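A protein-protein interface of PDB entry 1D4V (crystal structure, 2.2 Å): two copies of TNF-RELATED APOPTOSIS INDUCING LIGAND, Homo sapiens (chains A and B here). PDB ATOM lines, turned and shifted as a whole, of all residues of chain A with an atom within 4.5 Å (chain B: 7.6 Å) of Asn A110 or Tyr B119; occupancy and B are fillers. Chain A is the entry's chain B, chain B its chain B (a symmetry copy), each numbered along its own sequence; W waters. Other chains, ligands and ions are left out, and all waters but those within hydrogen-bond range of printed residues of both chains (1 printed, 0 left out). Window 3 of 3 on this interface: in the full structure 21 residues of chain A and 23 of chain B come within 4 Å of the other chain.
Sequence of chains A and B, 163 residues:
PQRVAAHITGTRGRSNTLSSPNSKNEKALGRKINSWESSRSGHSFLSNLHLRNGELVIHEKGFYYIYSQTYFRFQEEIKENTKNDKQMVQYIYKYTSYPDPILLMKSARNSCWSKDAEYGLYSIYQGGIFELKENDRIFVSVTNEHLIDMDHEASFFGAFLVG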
ATOM      1  N   ASP A  85      25.722  22.708   5.593  1.00  0.00           N
ATOM      2  CA  ASP A  85      25.766  21.268   5.805  1.00  0.00           C
ATOM      3  C   ASP A  85      24.317  20.976   6.141  1.00  0.00           C
ATOM      4  O   ASP A  85      23.845  21.331   7.222  1.00  0.00           O
ATOM      5  CB  ASP A  85      26.675  20.935   6.996  1.00  0.00           C
ATOM      6  CG  ASP A  85      27.799  19.977   6.630  1.00  0.00           C
ATOM      7  OD1 ASP A  85      28.131  19.877   5.426  1.00  0.00           O
ATOM      8  OD2 ASP A  85      28.365  19.339   7.551  1.00  0.00           O
ATOM      9  N   LYS A  86      23.601  20.356   5.212  1.00  0.00           N
ATOM     10  CA  LYS A  86      22.192  20.092   5.454  1.00  0.00           C
ATOM     11  C   LYS A  86      21.818  18.653   5.723  1.00  0.00           C
ATOM     12  O   LYS A  86      22.348  17.727   5.117  1.00  0.00           O
ATOM     13  CB  LYS A  86      21.362  20.615   4.291  1.00  0.00           C
ATOM     14  CG  LYS A  86      21.760  22.015   3.893  1.00  0.00           C
ATOM     15  CD  LYS A  86      20.993  22.522   2.688  1.00  0.00           C
ATOM     16  CE  LYS A  86      21.556  23.880   2.250  1.00  0.00           C
ATOM     17  NZ  LYS A  86      21.703  24.842   3.398  1.00  0.00           N
ATOM     18  N   GLN A  87      20.924  18.493   6.684  1.00  0.00           N
ATOM     19  CA  GLN A  87      20.380  17.191   7.030  1.00  0.00           C
ATOM     20  C   GLN A  87      18.971  17.198   6.445  1.00  0.00           C
ATOM     21  O   GLN A  87      18.131  18.012   6.831  1.00  0.00           O
ATOM     22  CB  GLN A  87      20.340  16.997   8.546  1.00  0.00           C
ATOM     23  CG  GLN A  87      21.724  16.747   9.172  1.00  0.00           C
ATOM     24  CD  GLN A  87      21.693  16.630  10.700  1.00  0.00           C
ATOM     25  OE1 GLN A  87      20.686  16.275  11.292  1.00  0.00           O
ATOM     26  NE2 GLN A  87      22.807  16.920  11.323  1.00  0.00           N
ATOM     27  N   MET A  88      18.738  16.310   5.482  1.00  0.00           N
ATOM     28  CA  MET A  88      17.446  16.187   4.803  1.00  0.00           C
ATOM     29  C   MET A  88      16.770  14.944   5.335  1.00  0.00           C
ATOM     30  O   MET A  88      17.195  13.821   5.063  1.00  0.00           O
ATOM     31  CB  MET A  88      17.692  16.104   3.302  1.00  0.00           C
ATOM     32  CG  MET A  88      18.163  17.438   2.770  1.00  0.00           C
ATOM     33  SD  MET A  88      18.985  17.405   1.206  1.00  0.00           S
ATOM     34  CE  MET A  88      20.525  16.626   1.573  1.00  0.00           C
ATOM     35  N   ARG A 109      19.283  11.971   4.607  1.00  0.00           N
ATOM     36  CA  ARG A 109      20.404  12.176   3.698  1.00  0.00           C
ATOM     37  C   ARG A 109      21.089  13.437   4.208  1.00  0.00           C
ATOM     38  O   ARG A 109      20.453  14.292   4.832  1.00  0.00           O
ATOM     39  CB  ARG A 109      19.938  12.447   2.266  1.00  0.00           C
ATOM     40  CG  ARG A 109      18.866  11.521   1.742  1.00  0.00           C
ATOM     41  CD  ARG A 109      19.317  10.097   1.412  1.00  0.00           C
ATOM     42  NE  ARG A 109      18.133   9.218   1.444  1.00  0.00           N
ATOM     43  CZ  ARG A 109      17.618   8.599   0.384  1.00  0.00           C
ATOM     44  NH1 ARG A 109      18.174   8.735  -0.813  1.00  0.00           N
ATOM     45  NH2 ARG A 109      16.518   7.865   0.508  1.00  0.00           N
ATOM     46  N   ASN A 110      22.384  13.554   3.964  1.00  0.00           N
ATOM     47  CA  ASN A 110      23.070  14.773   4.365  1.00  0.00           C
ATOM     48  C   ASN A 110      23.735  15.331   3.111  1.00  0.00           C
ATOM     49  O   ASN A 110      24.123  14.584   2.206  1.00  0.00           O
ATOM     50  CB  ASN A 110      24.092  14.505   5.482  1.00  0.00           C
ATOM     51  CG  ASN A 110      25.344  13.821   4.986  1.00  0.00           C
ATOM     52  OD1 ASN A 110      26.403  14.438   4.916  1.00  0.00           O
ATOM     53  ND2 ASN A 110      25.241  12.544   4.650  1.00  0.00           N
ATOM     54  N   SER A 111      23.820  16.641   3.012  1.00  0.00           N
ATOM     55  CA  SER A 111      24.468  17.221   1.833  1.00  0.00           C
ATOM     56  C   SER A 111      25.949  16.873   1.953  1.00  0.00           C
ATOM     57  O   SER A 111      26.435  16.658   3.055  1.00  0.00           O
ATOM     58  CB  SER A 111      24.282  18.727   1.828  1.00  0.00           C
ATOM     59  OG  SER A 111      24.743  19.284   3.053  1.00  0.00           O
ATOM     60  N   CYS A 112      26.685  16.821   0.850  1.00  0.00           N
ATOM     61  CA  CYS A 112      28.096  16.454   0.969  1.00  0.00           C
ATOM     62  C   CYS A 112      29.127  17.552   0.715  1.00  0.00           C
ATOM     63  O   CYS A 112      29.646  18.171   1.648  1.00  0.00           O
ATOM     64  CB  CYS A 112      28.404  15.270   0.054  1.00  0.00           C
ATOM     65  SG  CYS A 112      30.170  14.879  -0.045  1.00  0.00           S
ATOM     66  N   TYR A 122      18.032  15.735  -4.022  1.00  0.00           N
ATOM     67  CA  TYR A 122      17.869  14.577  -3.155  1.00  0.00           C
ATOM     68  C   TYR A 122      16.424  14.103  -3.031  1.00  0.00           C
ATOM     69  O   TYR A 122      15.672  14.644  -2.242  1.00  0.00           O
ATOM     70  CB  TYR A 122      18.428  14.855  -1.743  1.00  0.00           C
ATOM     71  CG  TYR A 122      19.939  15.095  -1.686  1.00  0.00           C
ATOM     72  CD1 TYR A 122      20.485  16.353  -1.983  1.00  0.00           C
ATOM     73  CD2 TYR A 122      20.823  14.057  -1.368  1.00  0.00           C
ATOM     74  CE1 TYR A 122      21.875  16.561  -1.967  1.00  0.00           C
ATOM     75  CE2 TYR A 122      22.218  14.256  -1.346  1.00  0.00           C
ATOM     76  CZ  TYR A 122      22.730  15.511  -1.650  1.00  0.00           C
ATOM     77  OH  TYR A 122      24.095  15.718  -1.654  1.00  0.00           O
ATOM     78  N   PHE B  72      22.487   3.864   7.270  1.00  0.00           N
ATOM     79  CA  PHE B  72      23.909   3.925   7.526  1.00  0.00           C
ATOM     80  C   PHE B  72      24.063   5.300   8.068  1.00  0.00           C
ATOM     81  O   PHE B  72      23.740   6.272   7.389  1.00  0.00           O
ATOM     82  CB  PHE B  72      24.686   3.768   6.235  1.00  0.00           C
ATOM     83  CG  PHE B  72      24.676   2.371   5.703  1.00  0.00           C
ATOM     84  CD1 PHE B  72      25.698   1.480   6.033  1.00  0.00           C
ATOM     85  CD2 PHE B  72      23.663   1.946   4.840  1.00  0.00           C
ATOM     86  CE1 PHE B  72      25.715   0.189   5.498  1.00  0.00           C
ATOM     87  CE2 PHE B  72      23.680   0.663   4.301  1.00  0.00           C
ATOM     88  CZ  PHE B  72      24.709  -0.213   4.629  1.00  0.00           C
ATOM     89  N   ARG B  73      24.515   5.372   9.314  1.00  0.00           N
ATOM     90  CA  ARG B  73      24.703   6.638  10.027  1.00  0.00           C
ATOM     91  C   ARG B  73      26.053   6.575  10.716  1.00  0.00           C
ATOM     92  O   ARG B  73      26.298   5.679  11.523  1.00  0.00           O
ATOM     93  CB  ARG B  73      23.608   6.814  11.088  1.00  0.00           C
ATOM     94  CG  ARG B  73      23.725   8.095  11.911  1.00  0.00           C
ATOM     95  CD  ARG B  73      22.393   8.483  12.557  1.00  0.00           C
ATOM     96  NE  ARG B  73      22.261   7.965  13.904  1.00  0.00           N
ATOM     97  CZ  ARG B  73      22.671   8.602  14.997  1.00  0.00           C
ATOM     98  NH1 ARG B  73      23.240   9.792  14.908  1.00  0.00           N
ATOM     99  NH2 ARG B  73      22.510   8.043  16.190  1.00  0.00           N
ATOM    100  N   PHE B  74      26.936   7.513  10.399  1.00  0.00           N
ATOM    101  CA  PHE B  74      28.250   7.490  11.012  1.00  0.00           C
ATOM    102  C   PHE B  74      28.918   8.859  11.096  1.00  0.00           C
ATOM    103  O   PHE B  74      28.762   9.717  10.221  1.00  0.00           O
ATOM    104  CB  PHE B  74      29.136   6.539  10.224  1.00  0.00           C
ATOM    105  CG  PHE B  74      29.395   7.002   8.827  1.00  0.00           C
ATOM    106  CD1 PHE B  74      30.383   7.940   8.572  1.00  0.00           C
ATOM    107  CD2 PHE B  74      28.599   6.568   7.778  1.00  0.00           C
ATOM    108  CE1 PHE B  74      30.574   8.447   7.295  1.00  0.00           C
ATOM    109  CE2 PHE B  74      28.787   7.071   6.493  1.00  0.00           C
ATOM    110  CZ  PHE B  74      29.771   8.009   6.256  1.00  0.00           C
ATOM    111  N   GLN B  75      29.663   9.050  12.174  1.00  0.00           N
ATOM    112  CA  GLN B  75      30.402  10.283  12.398  1.00  0.00           C
ATOM    113  C   GLN B  75      31.794   9.822  11.990  1.00  0.00           C
ATOM    114  O   GLN B  75      32.200   8.718  12.343  1.00  0.00           O
ATOM    115  CB  GLN B  75      30.344  10.658  13.885  1.00  0.00           C
ATOM    116  CG  GLN B  75      30.874  12.039  14.250  1.00  0.00           C
ATOM    117  CD  GLN B  75      29.832  12.906  14.970  1.00  0.00           C
ATOM    118  OE1 GLN B  75      29.059  12.420  15.805  1.00  0.00           O
ATOM    119  NE2 GLN B  75      29.817  14.200  14.649  1.00  0.00           N
ATOM    120  N   GLU B  76      32.517  10.618  11.218  1.00  0.00           N
ATOM    121  CA  GLU B  76      33.842  10.177  10.820  1.00  0.00           C
ATOM    122  C   GLU B  76      34.932  11.219  11.009  1.00  0.00           C
ATOM    123  O   GLU B  76      34.741  12.399  10.717  1.00  0.00           O
ATOM    124  CB  GLU B  76      33.833   9.727   9.364  1.00  0.00           C
ATOM    125  CG  GLU B  76      33.671  10.857   8.380  1.00  0.00           C
ATOM    126  CD  GLU B  76      34.058  10.448   6.977  1.00  0.00           C
ATOM    127  OE1 GLU B  76      33.993  11.303   6.075  1.00  0.00           O
ATOM    128  OE2 GLU B  76      34.433   9.272   6.776  1.00  0.00           O
ATOM    129  N   GLU B  77      36.075  10.761  11.506  1.00  0.00           N
ATOM    130  CA  GLU B  77      37.233  11.620  11.721  1.00  0.00           C
ATOM    131  C   GLU B  77      38.383  11.047  10.902  1.00  0.00           C
ATOM    132  O   GLU B  77      39.145  10.207  11.385  1.00  0.00           O
ATOM    133  CB  GLU B  77      37.612  11.664  13.211  1.00  0.00           C
ATOM    134  CG  GLU B  77      38.969  12.318  13.510  1.00  0.00           C
ATOM    135  CD  GLU B  77      38.873  13.591  14.353  1.00  0.00           C
ATOM    136  OE1 GLU B  77      38.414  14.633  13.834  1.00  0.00           O
ATOM    137  OE2 GLU B  77      39.260  13.545  15.541  1.00  0.00           O
ATOM    138  N   TRP B 113      32.376  13.152  -0.112  1.00  0.00           N
ATOM    139  CA  TRP B 113      33.342  14.113   0.415  1.00  0.00           C
ATOM    140  C   TRP B 113      34.817  13.696   0.510  1.00  0.00           C
ATOM    141  O   TRP B 113      35.542  13.731  -0.487  1.00  0.00           O
ATOM    142  CB  TRP B 113      32.847  14.601   1.789  1.00  0.00           C
ATOM    143  CG  TRP B 113      31.842  13.672   2.496  1.00  0.00           C
ATOM    144  CD1 TRP B 113      30.548  13.974   2.849  1.00  0.00           C
ATOM    145  CD2 TRP B 113      32.079  12.335   2.971  1.00  0.00           C
ATOM    146  NE1 TRP B 113      29.974  12.914   3.514  1.00  0.00           N
ATOM    147  CE2 TRP B 113      30.888  11.897   3.604  1.00  0.00           C
ATOM    148  CE3 TRP B 113      33.183  11.465   2.928  1.00  0.00           C
ATOM    149  CZ2 TRP B 113      30.771  10.629   4.190  1.00  0.00           C
ATOM    150  CZ3 TRP B 113      33.065  10.201   3.513  1.00  0.00           C
ATOM    151  CH2 TRP B 113      31.866   9.798   4.135  1.00  0.00           C
ATOM    152  N   ASP B 116      37.686  16.671   4.344  1.00  0.00           N
ATOM    153  CA  ASP B 116      36.806  17.732   4.812  1.00  0.00           C
ATOM    154  C   ASP B 116      35.356  17.231   4.809  1.00  0.00           C
ATOM    155  O   ASP B 116      34.599  17.506   3.878  1.00  0.00           O
ATOM    156  CB  ASP B 116      36.950  18.955   3.898  1.00  0.00           C
ATOM    157  CG  ASP B 116      36.211  20.173   4.420  1.00  0.00           C
ATOM    158  OD1 ASP B 116      36.491  20.588   5.567  1.00  0.00           O
ATOM    159  OD2 ASP B 116      35.356  20.714   3.680  1.00  0.00           O
ATOM    160  N   ALA B 117      34.979  16.490   5.851  1.00  0.00           N
ATOM    161  CA  ALA B 117      33.630  15.943   5.971  1.00  0.00           C
ATOM    162  C   ALA B 117      33.434  15.416   7.372  1.00  0.00           C
ATOM    163  O   ALA B 117      34.181  14.550   7.823  1.00  0.00           O
ATOM    164  CB  ALA B 117      33.438  14.822   4.986  1.00  0.00           C
ATOM    165  N   GLU B 118      32.410  15.910   8.053  1.00  0.00           N
ATOM    166  CA  GLU B 118      32.171  15.485   9.420  1.00  0.00           C
ATOM    167  C   GLU B 118      31.337  14.218   9.642  1.00  0.00           C
ATOM    168  O   GLU B 118      31.594  13.493  10.593  1.00  0.00           O
ATOM    169  CB  GLU B 118      31.553  16.633  10.226  1.00  0.00           C
ATOM    170  CG  GLU B 118      31.123  16.193  11.617  1.00  0.00           C
ATOM    171  CD  GLU B 118      30.318  17.233  12.369  1.00  0.00           C
ATOM    172  OE1 GLU B 118      29.733  16.855  13.412  1.00  0.00           O
ATOM    173  OE2 GLU B 118      30.272  18.410  11.934  1.00  0.00           O
ATOM    174  N   TYR B 119      30.343  13.945   8.794  1.00  0.00           N
ATOM    175  CA  TYR B 119      29.507  12.758   8.984  1.00  0.00           C
ATOM    176  C   TYR B 119      28.692  12.339   7.759  1.00  0.00           C
ATOM    177  O   TYR B 119      28.639  13.040   6.741  1.00  0.00           O
ATOM    178  CB  TYR B 119      28.555  12.970  10.177  1.00  0.00           C
ATOM    179  CG  TYR B 119      27.614  14.142  10.011  1.00  0.00           C
ATOM    180  CD1 TYR B 119      26.517  14.069   9.160  1.00  0.00           C
ATOM    181  CD2 TYR B 119      27.873  15.360  10.646  1.00  0.00           C
ATOM    182  CE1 TYR B 119      25.701  15.189   8.934  1.00  0.00           C
ATOM    183  CE2 TYR B 119      27.061  16.483  10.425  1.00  0.00           C
ATOM    184  CZ  TYR B 119      25.985  16.390   9.568  1.00  0.00           C
ATOM    185  OH  TYR B 119      25.205  17.504   9.337  1.00  0.00           O
ATOM    186  N   GLY B 120      28.040  11.189   7.875  1.00  0.00           N
ATOM    187  CA  GLY B 120      27.244  10.700   6.767  1.00  0.00           C
ATOM    188  C   GLY B 120      25.925  10.099   7.192  1.00  0.00           C
ATOM    189  O   GLY B 120      25.844   9.340   8.160  1.00  0.00           O
ATOM    190  N   LEU B 121      24.877  10.453   6.461  1.00  0.00           N
ATOM    191  CA  LEU B 121      23.552   9.922   6.710  1.00  0.00           C
ATOM    192  C   LEU B 121      23.082   9.275   5.410  1.00  0.00           C
ATOM    193  O   LEU B 121      22.812   9.965   4.426  1.00  0.00           O
ATOM    194  CB  LEU B 121      22.593  11.048   7.108  1.00  0.00           C
ATOM    195  CG  LEU B 121      22.994  11.926   8.302  1.00  0.00           C
ATOM    196  CD1 LEU B 121      21.884  12.936   8.603  1.00  0.00           C
ATOM    197  CD2 LEU B 121      23.228  11.077   9.511  1.00  0.00           C
ATOM    198  N   TYR B 122      22.962   7.955   5.399  1.00  0.00           N
ATOM    199  CA  TYR B 122      22.498   7.287   4.190  1.00  0.00           C
ATOM    200  C   TYR B 122      21.423   6.234   4.447  1.00  0.00           C
ATOM    201  O   TYR B 122      21.740   5.113   4.796  1.00  0.00           O
ATOM    202  CB  TYR B 122      23.671   6.630   3.431  1.00  0.00           C
ATOM    203  CG  TYR B 122      24.710   7.612   2.883  1.00  0.00           C
ATOM    204  CD1 TYR B 122      25.728   8.122   3.703  1.00  0.00           C
ATOM    205  CD2 TYR B 122      24.655   8.053   1.555  1.00  0.00           C
ATOM    206  CE1 TYR B 122      26.658   9.052   3.207  1.00  0.00           C
ATOM    207  CE2 TYR B 122      25.586   8.982   1.048  1.00  0.00           C
ATOM    208  CZ  TYR B 122      26.579   9.475   1.883  1.00  0.00           C
ATOM    209  OH  TYR B 122      27.484  10.402   1.410  1.00  0.00           O
ATOM    210  N   SER B 123      20.147   6.599   4.291  1.00  0.00           N
ATOM    211  CA  SER B 123      19.073   5.612   4.440  1.00  0.00           C
ATOM    212  C   SER B 123      18.891   4.970   3.067  1.00  0.00           C
ATOM    213  O   SER B 123      18.780   5.669   2.050  1.00  0.00           O
ATOM    214  CB  SER B 123      17.727   6.248   4.860  1.00  0.00           C
ATOM    215  OG  SER B 123      17.790   6.842   6.153  1.00  0.00           O
HETATM  216  O   HOH W   1      29.287  16.398   6.242  1.00  0.00           O
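1 position is printed for both chains.
Of the 8 pairs that touch across the chains among the printed residues, none has its exchanged pair printed and touching as well.
The side-chain amide nitrogen of Asn A110 lies close to the backbone NH of Leu B121 (2.8 Å).
The side-chain sulfur of Cys A112 is in hydrogen-bond range of the backbone NH of Trp B113, 2.8 Å away.
OD1 of Asn A110 sits close to O of Tyr B119, 3.2 Å away.
The side-chain amide nitrogen of Gln A87 sits at hydrogen-bond distance from the side-chain hydroxyl of Tyr B119.
Of the printed residues of chain B, Gln A87 touches Tyr B119 and Leu B121.
Asn A110 touches just these residues of chain B: Tyr B119, Gly B120 and Leu B121.
Printed residues of chain B within 4 Å of Cys A112: Trp B113 (2.8 Å).
Of chain A, only Gln A87 (3.2 Å) and Asn A110 (3.2 Å) come within 4 Å of Tyr B119.
Of the printed residues of chain A, Gly B120 touches Asn A110 (3.4 Å).
Of the printed residues of chain A, Leu B121 touches Gln A87 (3.9 Å), Arg A109 (3.3 Å) and Asn A110 (2.8 Å).
The nearest residue of chain A that does not touch Tyr B119 is Asp A85 (4.1 Å).
The nearest printed residue of chain A that does not touch Trp B113 is Asn A110 (4.1 Å).
Of the 15 printed residues of chain B, 5 touch a printed residue of chain A.
Hydrophobic or aromatic side chains of chain B within 4 Å of the printed part of chain A: Trp B113, Tyr B119 and Leu B121.
Among the printed residues, 8 pairs touch across the chains.
Among the printed residues, no Asp or Glu carboxylate lies within 4 Å of a Lys or Arg side-chain nitrogen of the other chain.
Water W1 lies within hydrogen-bond range of the side-chain carboxylate of Asp A85 and the backbone carbonyl oxygen of Tyr B119.
The backbone NH of Gly B120 is in hydrogen-bond range of the backbone carbonyl oxygen of Phe B74, 2.9 Å away.
The backbone NH of Met A88 is in hydrogen-bond range of the backbone carbonyl oxygen of Arg A109 (2.7 Å).
NE1 of Trp B113 sits at hydrogen-bond distance from O of Tyr B119 (3.5 Å).
Among the printed residues, pairs that only touch across the chains: Gln A87 with Leu B121, Arg A109 with Leu B121, Arg A109 with Ser B123 and Asn A110 with Gly B120.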
